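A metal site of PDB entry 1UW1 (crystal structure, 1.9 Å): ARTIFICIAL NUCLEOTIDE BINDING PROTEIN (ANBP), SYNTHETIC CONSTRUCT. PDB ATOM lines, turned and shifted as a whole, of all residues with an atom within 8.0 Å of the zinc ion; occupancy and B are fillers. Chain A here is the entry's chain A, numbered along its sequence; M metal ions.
SG of Cys 28 sits close to N of Ala 31, 3.4 Å away. SG of Cys 28 lies close to N of Val 30 (3.7 Å). The side-chain sulfur (SG) of Cys 48 sits close to the backbone NH (N) of Thr 50, 3.7 Å away. N of Cys 25 is in hydrogen-bond range of O of Ala 31, 2.8 Å away. SG of Cys 25 sits close to N of Lys 27, 3.4 Å away.
Four residues have an atom within 4 Å of the zinc ion: Cys 25, Cys 28, Cys 48 and Cys 51. The nearest printed residue that does not touch the zinc ion is Ala 31 (4.4 Å).
The zinc ion is bound by SG of Cys 51, 2.4 Å away. SG of Cys 28 is bound to the zinc ion, 2.4 Å away. SG of Cys 48 is bound to the zinc ion, 2.5 Å away. SG of Cys 25 binds the zinc ion (2.5 Å). The zinc ion has four donor atoms within binding distance.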
ATOM      1  N   PRO A  24     -23.933  -0.065 -19.029  1.00  0.00           N
ATOM      2  CA  PRO A  24     -24.645  -1.161 -18.391  1.00  0.00           C
ATOM      3  C   PRO A  24     -23.705  -2.337 -18.164  1.00  0.00           C
ATOM      4  O   PRO A  24     -22.635  -2.437 -18.771  1.00  0.00           O
ATOM      5  CB  PRO A  24     -25.705  -1.536 -19.433  1.00  0.00           C
ATOM      6  CG  PRO A  24     -25.769  -0.402 -20.323  1.00  0.00           C
ATOM      7  CD  PRO A  24     -24.439   0.181 -20.390  1.00  0.00           C
ATOM      8  N   CYS A  25     -24.130  -3.219 -17.256  1.00  0.00           N
ATOM      9  CA  CYS A  25     -23.458  -4.462 -16.948  1.00  0.00           C
ATOM     10  C   CYS A  25     -23.090  -5.179 -18.240  1.00  0.00           C
ATOM     11  O   CYS A  25     -23.907  -5.283 -19.147  1.00  0.00           O
ATOM     12  CB  CYS A  25     -24.423  -5.337 -16.135  1.00  0.00           C
ATOM     13  SG  CYS A  25     -23.900  -7.007 -15.929  1.00  0.00           S
ATOM     14  N   VAL A  26     -21.863  -5.679 -18.313  1.00  0.00           N
ATOM     15  CA  VAL A  26     -21.354  -6.300 -19.525  1.00  0.00           C
ATOM     16  C   VAL A  26     -22.022  -7.676 -19.826  1.00  0.00           C
ATOM     17  O   VAL A  26     -22.010  -8.128 -20.947  1.00  0.00           O
ATOM     18  CB  VAL A  26     -19.814  -6.511 -19.491  1.00  0.00           C
ATOM     19  CG1 VAL A  26     -19.092  -5.239 -19.325  1.00  0.00           C
ATOM     20  CG2 VAL A  26     -19.390  -7.534 -18.429  1.00  0.00           C
ATOM     21  N   LYS A  27     -22.635  -8.290 -18.819  1.00  0.00           N
ATOM     22  CA  LYS A  27     -23.255  -9.559 -18.960  1.00  0.00           C
ATOM     23  C   LYS A  27     -24.718  -9.467 -19.353  1.00  0.00           C
ATOM     24  O   LYS A  27     -25.119 -10.030 -20.365  1.00  0.00           O
ATOM     25  CB  LYS A  27     -23.093 -10.350 -17.655  1.00  0.00           C
ATOM     26  CG  LYS A  27     -23.568 -11.769 -17.685  1.00  0.00           C
ATOM     27  CD  LYS A  27     -22.725 -12.644 -18.558  1.00  0.00           C
ATOM     28  CE  LYS A  27     -23.429 -13.884 -18.982  1.00  0.00           C
ATOM     29  NZ  LYS A  27     -22.618 -14.726 -19.877  1.00  0.00           N
ATOM     30  N   CYS A  28     -25.544  -8.829 -18.532  1.00  0.00           N
ATOM     31  CA  CYS A  28     -26.974  -8.734 -18.802  1.00  0.00           C
ATOM     32  C   CYS A  28     -27.335  -7.561 -19.686  1.00  0.00           C
ATOM     33  O   CYS A  28     -28.460  -7.493 -20.181  1.00  0.00           O
ATOM     34  CB  CYS A  28     -27.804  -8.646 -17.526  1.00  0.00           C
ATOM     35  SG  CYS A  28     -27.695  -7.106 -16.545  1.00  0.00           S
ATOM     36  N   LYS A  29     -26.386  -6.637 -19.866  1.00  0.00           N
ATOM     37  CA  LYS A  29     -26.543  -5.479 -20.731  1.00  0.00           C
ATOM     38  C   LYS A  29     -27.706  -4.513 -20.409  1.00  0.00           C
ATOM     39  O   LYS A  29     -27.980  -3.630 -21.179  1.00  0.00           O
ATOM     40  CB  LYS A  29     -26.624  -5.950 -22.187  1.00  0.00           C
ATOM     41  CG  LYS A  29     -25.728  -7.109 -22.484  1.00  0.00           C
ATOM     42  CD  LYS A  29     -24.926  -6.986 -23.711  1.00  0.00           C
ATOM     43  CE  LYS A  29     -24.140  -8.274 -23.965  1.00  0.00           C
ATOM     44  NZ  LYS A  29     -24.212  -8.637 -25.421  1.00  0.00           N
ATOM     45  N   VAL A  30     -28.341  -4.663 -19.267  1.00  0.00           N
ATOM     46  CA  VAL A  30     -29.438  -3.803 -18.864  1.00  0.00           C
ATOM     47  C   VAL A  30     -29.157  -3.095 -17.533  1.00  0.00           C
ATOM     48  O   VAL A  30     -29.228  -1.868 -17.452  1.00  0.00           O
ATOM     49  CB  VAL A  30     -30.736  -4.606 -18.749  1.00  0.00           C
ATOM     50  CG1 VAL A  30     -31.819  -3.776 -18.121  1.00  0.00           C
ATOM     51  CG2 VAL A  30     -31.167  -5.076 -20.136  1.00  0.00           C
ATOM     52  N   ALA A  31     -28.805  -3.844 -16.515  1.00  0.00           N
ATOM     53  CA  ALA A  31     -28.642  -3.277 -15.176  1.00  0.00           C
ATOM     54  C   ALA A  31     -27.401  -2.420 -15.102  1.00  0.00           C
ATOM     55  O   ALA A  31     -26.441  -2.624 -15.849  1.00  0.00           O
ATOM     56  CB  ALA A  31     -28.603  -4.420 -14.135  1.00  0.00           C
ATOM     57  N   PRO A  32     -27.385  -1.435 -14.204  1.00  0.00           N
ATOM     58  CA  PRO A  32     -26.154  -0.687 -13.929  1.00  0.00           C
ATOM     59  C   PRO A  32     -25.139  -1.534 -13.222  1.00  0.00           C
ATOM     60  O   PRO A  32     -25.474  -2.561 -12.631  1.00  0.00           O
ATOM     61  CB  PRO A  32     -26.638   0.482 -13.051  1.00  0.00           C
ATOM     62  CG  PRO A  32     -28.051   0.368 -12.957  1.00  0.00           C
ATOM     63  CD  PRO A  32     -28.501  -0.931 -13.401  1.00  0.00           C
ATOM     64  N   ARG A  33     -23.873  -1.154 -13.328  1.00  0.00           N
ATOM     65  CA  ARG A  33     -22.780  -1.855 -12.700  1.00  0.00           C
ATOM     66  C   ARG A  33     -22.689  -1.699 -11.182  1.00  0.00           C
ATOM     67  O   ARG A  33     -23.087  -0.689 -10.619  1.00  0.00           O
ATOM     68  CB  ARG A  33     -21.451  -1.442 -13.353  1.00  0.00           C
ATOM     69  CG  ARG A  33     -21.404  -1.753 -14.824  1.00  0.00           C
ATOM     70  CD  ARG A  33     -20.233  -1.151 -15.585  1.00  0.00           C
ATOM     71  NE  ARG A  33     -20.287  -1.560 -16.977  1.00  0.00           N
ATOM     72  CZ  ARG A  33     -19.232  -1.917 -17.720  1.00  0.00           C
ATOM     73  NH1 ARG A  33     -18.017  -1.865 -17.263  1.00  0.00           N
ATOM     74  NH2 ARG A  33     -19.418  -2.239 -18.957  1.00  0.00           N
ATOM     75  N   ASN A  34     -22.141  -2.708 -10.500  1.00  0.00           N
ATOM     76  CA  ASN A  34     -21.766  -2.537  -9.140  1.00  0.00           C
ATOM     77  C   ASN A  34     -20.548  -1.639  -9.124  1.00  0.00           C
ATOM     78  O   ASN A  34     -19.841  -1.493 -10.126  1.00  0.00           O
ATOM     79  CB  ASN A  34     -21.496  -3.835  -8.460  1.00  0.00           C
ATOM     80  CG  ASN A  34     -21.512  -3.709  -6.964  1.00  0.00           C
ATOM     81  OD1 ASN A  34     -22.215  -2.863  -6.392  1.00  0.00           O
ATOM     82  ND2 ASN A  34     -20.774  -4.583  -6.320  1.00  0.00           N
ATOM     83  N   ASN A  46     -17.310  -4.617 -13.676  1.00  0.00           N
ATOM     84  CA  ASN A  46     -17.795  -4.843 -15.029  1.00  0.00           C
ATOM     85  C   ASN A  46     -19.272  -5.261 -15.011  1.00  0.00           C
ATOM     86  O   ASN A  46     -19.981  -5.072 -15.959  1.00  0.00           O
ATOM     87  CB  ASN A  46     -16.998  -5.900 -15.801  1.00  0.00           C
ATOM     88  CG  ASN A  46     -15.587  -5.456 -16.205  1.00  0.00           C
ATOM     89  OD1 ASN A  46     -15.241  -4.282 -16.252  1.00  0.00           O
ATOM     90  ND2 ASN A  46     -14.758  -6.442 -16.476  1.00  0.00           N
ATOM     91  N   MET A  47     -19.717  -5.858 -13.931  1.00  0.00           N
ATOM     92  CA  MET A  47     -21.056  -6.415 -13.851  1.00  0.00           C
ATOM     93  C   MET A  47     -21.841  -5.871 -12.695  1.00  0.00           C
ATOM     94  O   MET A  47     -21.287  -5.367 -11.757  1.00  0.00           O
ATOM     95  CB  MET A  47     -21.062  -7.937 -13.709  1.00  0.00           C
ATOM     96  CG  MET A  47     -20.558  -8.697 -14.927  1.00  0.00           C
ATOM     97  SD  MET A  47     -20.577 -10.492 -14.711  1.00  0.00           S
ATOM     98  CE  MET A  47     -19.140 -10.668 -13.757  1.00  0.00           C
ATOM     99  N   CYS A  48     -23.157  -6.048 -12.790  1.00  0.00           N
ATOM    100  CA  CYS A  48     -24.058  -5.727 -11.694  1.00  0.00           C
ATOM    101  C   CYS A  48     -23.867  -6.792 -10.627  1.00  0.00           C
ATOM    102  O   CYS A  48     -23.123  -7.738 -10.851  1.00  0.00           O
ATOM    103  CB  CYS A  48     -25.514  -5.727 -12.159  1.00  0.00           C
ATOM    104  SG  CYS A  48     -26.258  -7.257 -12.639  1.00  0.00           S
ATOM    105  N   LYS A  49     -24.442  -6.571  -9.456  1.00  0.00           N
ATOM    106  CA  LYS A  49     -24.256  -7.496  -8.343  1.00  0.00           C
ATOM    107  C   LYS A  49     -24.892  -8.881  -8.650  1.00  0.00           C
ATOM    108  O   LYS A  49     -24.282  -9.899  -8.402  1.00  0.00           O
ATOM    109  CB  LYS A  49     -24.792  -6.904  -7.065  1.00  0.00           C
ATOM    110  CG  LYS A  49     -24.633  -7.844  -5.841  1.00  0.00           C
ATOM    111  CD  LYS A  49     -23.197  -8.051  -5.474  1.00  0.00           C
ATOM    112  CE  LYS A  49     -23.141  -8.641  -4.057  1.00  0.00           C
ATOM    113  NZ  LYS A  49     -21.843  -8.435  -3.414  1.00  0.00           N
ATOM    114  N   THR A  50     -26.054  -8.890  -9.285  1.00  0.00           N
ATOM    115  CA  THR A  50     -26.726 -10.133  -9.627  1.00  0.00           C
ATOM    116  C   THR A  50     -25.878 -10.989 -10.561  1.00  0.00           C
ATOM    117  O   THR A  50     -25.674 -12.157 -10.315  1.00  0.00           O
ATOM    118  CB  THR A  50     -28.061  -9.843 -10.290  1.00  0.00           C
ATOM    119  OG1 THR A  50     -28.882  -9.156  -9.370  1.00  0.00           O
ATOM    120  CG2 THR A  50     -28.799 -11.152 -10.642  1.00  0.00           C
ATOM    121  N   CYS A  51     -25.409 -10.419 -11.640  1.00  0.00           N
ATOM    122  CA  CYS A  51     -24.578 -11.146 -12.617  1.00  0.00           C
ATOM    123  C   CYS A  51     -23.219 -11.604 -12.023  1.00  0.00           C
ATOM    124  O   CYS A  51     -22.776 -12.728 -12.229  1.00  0.00           O
ATOM    125  CB  CYS A  51     -24.422 -10.307 -13.898  1.00  0.00           C
ATOM    126  SG  CYS A  51     -25.942 -10.237 -14.863  1.00  0.00           S
ATOM    127  N   PHE A  52     -22.573 -10.760 -11.219  1.00  0.00           N
ATOM    128  CA  PHE A  52     -21.356 -11.150 -10.532  1.00  0.00           C
ATOM    129  C   PHE A  52     -21.603 -12.325  -9.602  1.00  0.00           C
ATOM    130  O   PHE A  52     -20.874 -13.307  -9.686  1.00  0.00           O
ATOM    131  CB  PHE A  52     -20.710  -9.994  -9.800  1.00  0.00           C
ATOM    132  CG  PHE A  52     -19.476 -10.392  -9.032  1.00  0.00           C
ATOM    133  CD1 PHE A  52     -18.310 -10.720  -9.699  1.00  0.00           C
ATOM    134  CD2 PHE A  52     -19.504 -10.471  -7.657  1.00  0.00           C
ATOM    135  CE1 PHE A  52     -17.171 -11.110  -8.976  1.00  0.00           C
ATOM    136  CE2 PHE A  52     -18.387 -10.837  -6.952  1.00  0.00           C
ATOM    137  CZ  PHE A  52     -17.228 -11.187  -7.628  1.00  0.00           C
HETATM  138 ZN    ZN M   1     -26.014  -7.848 -15.005  1.00  0.00          ZN
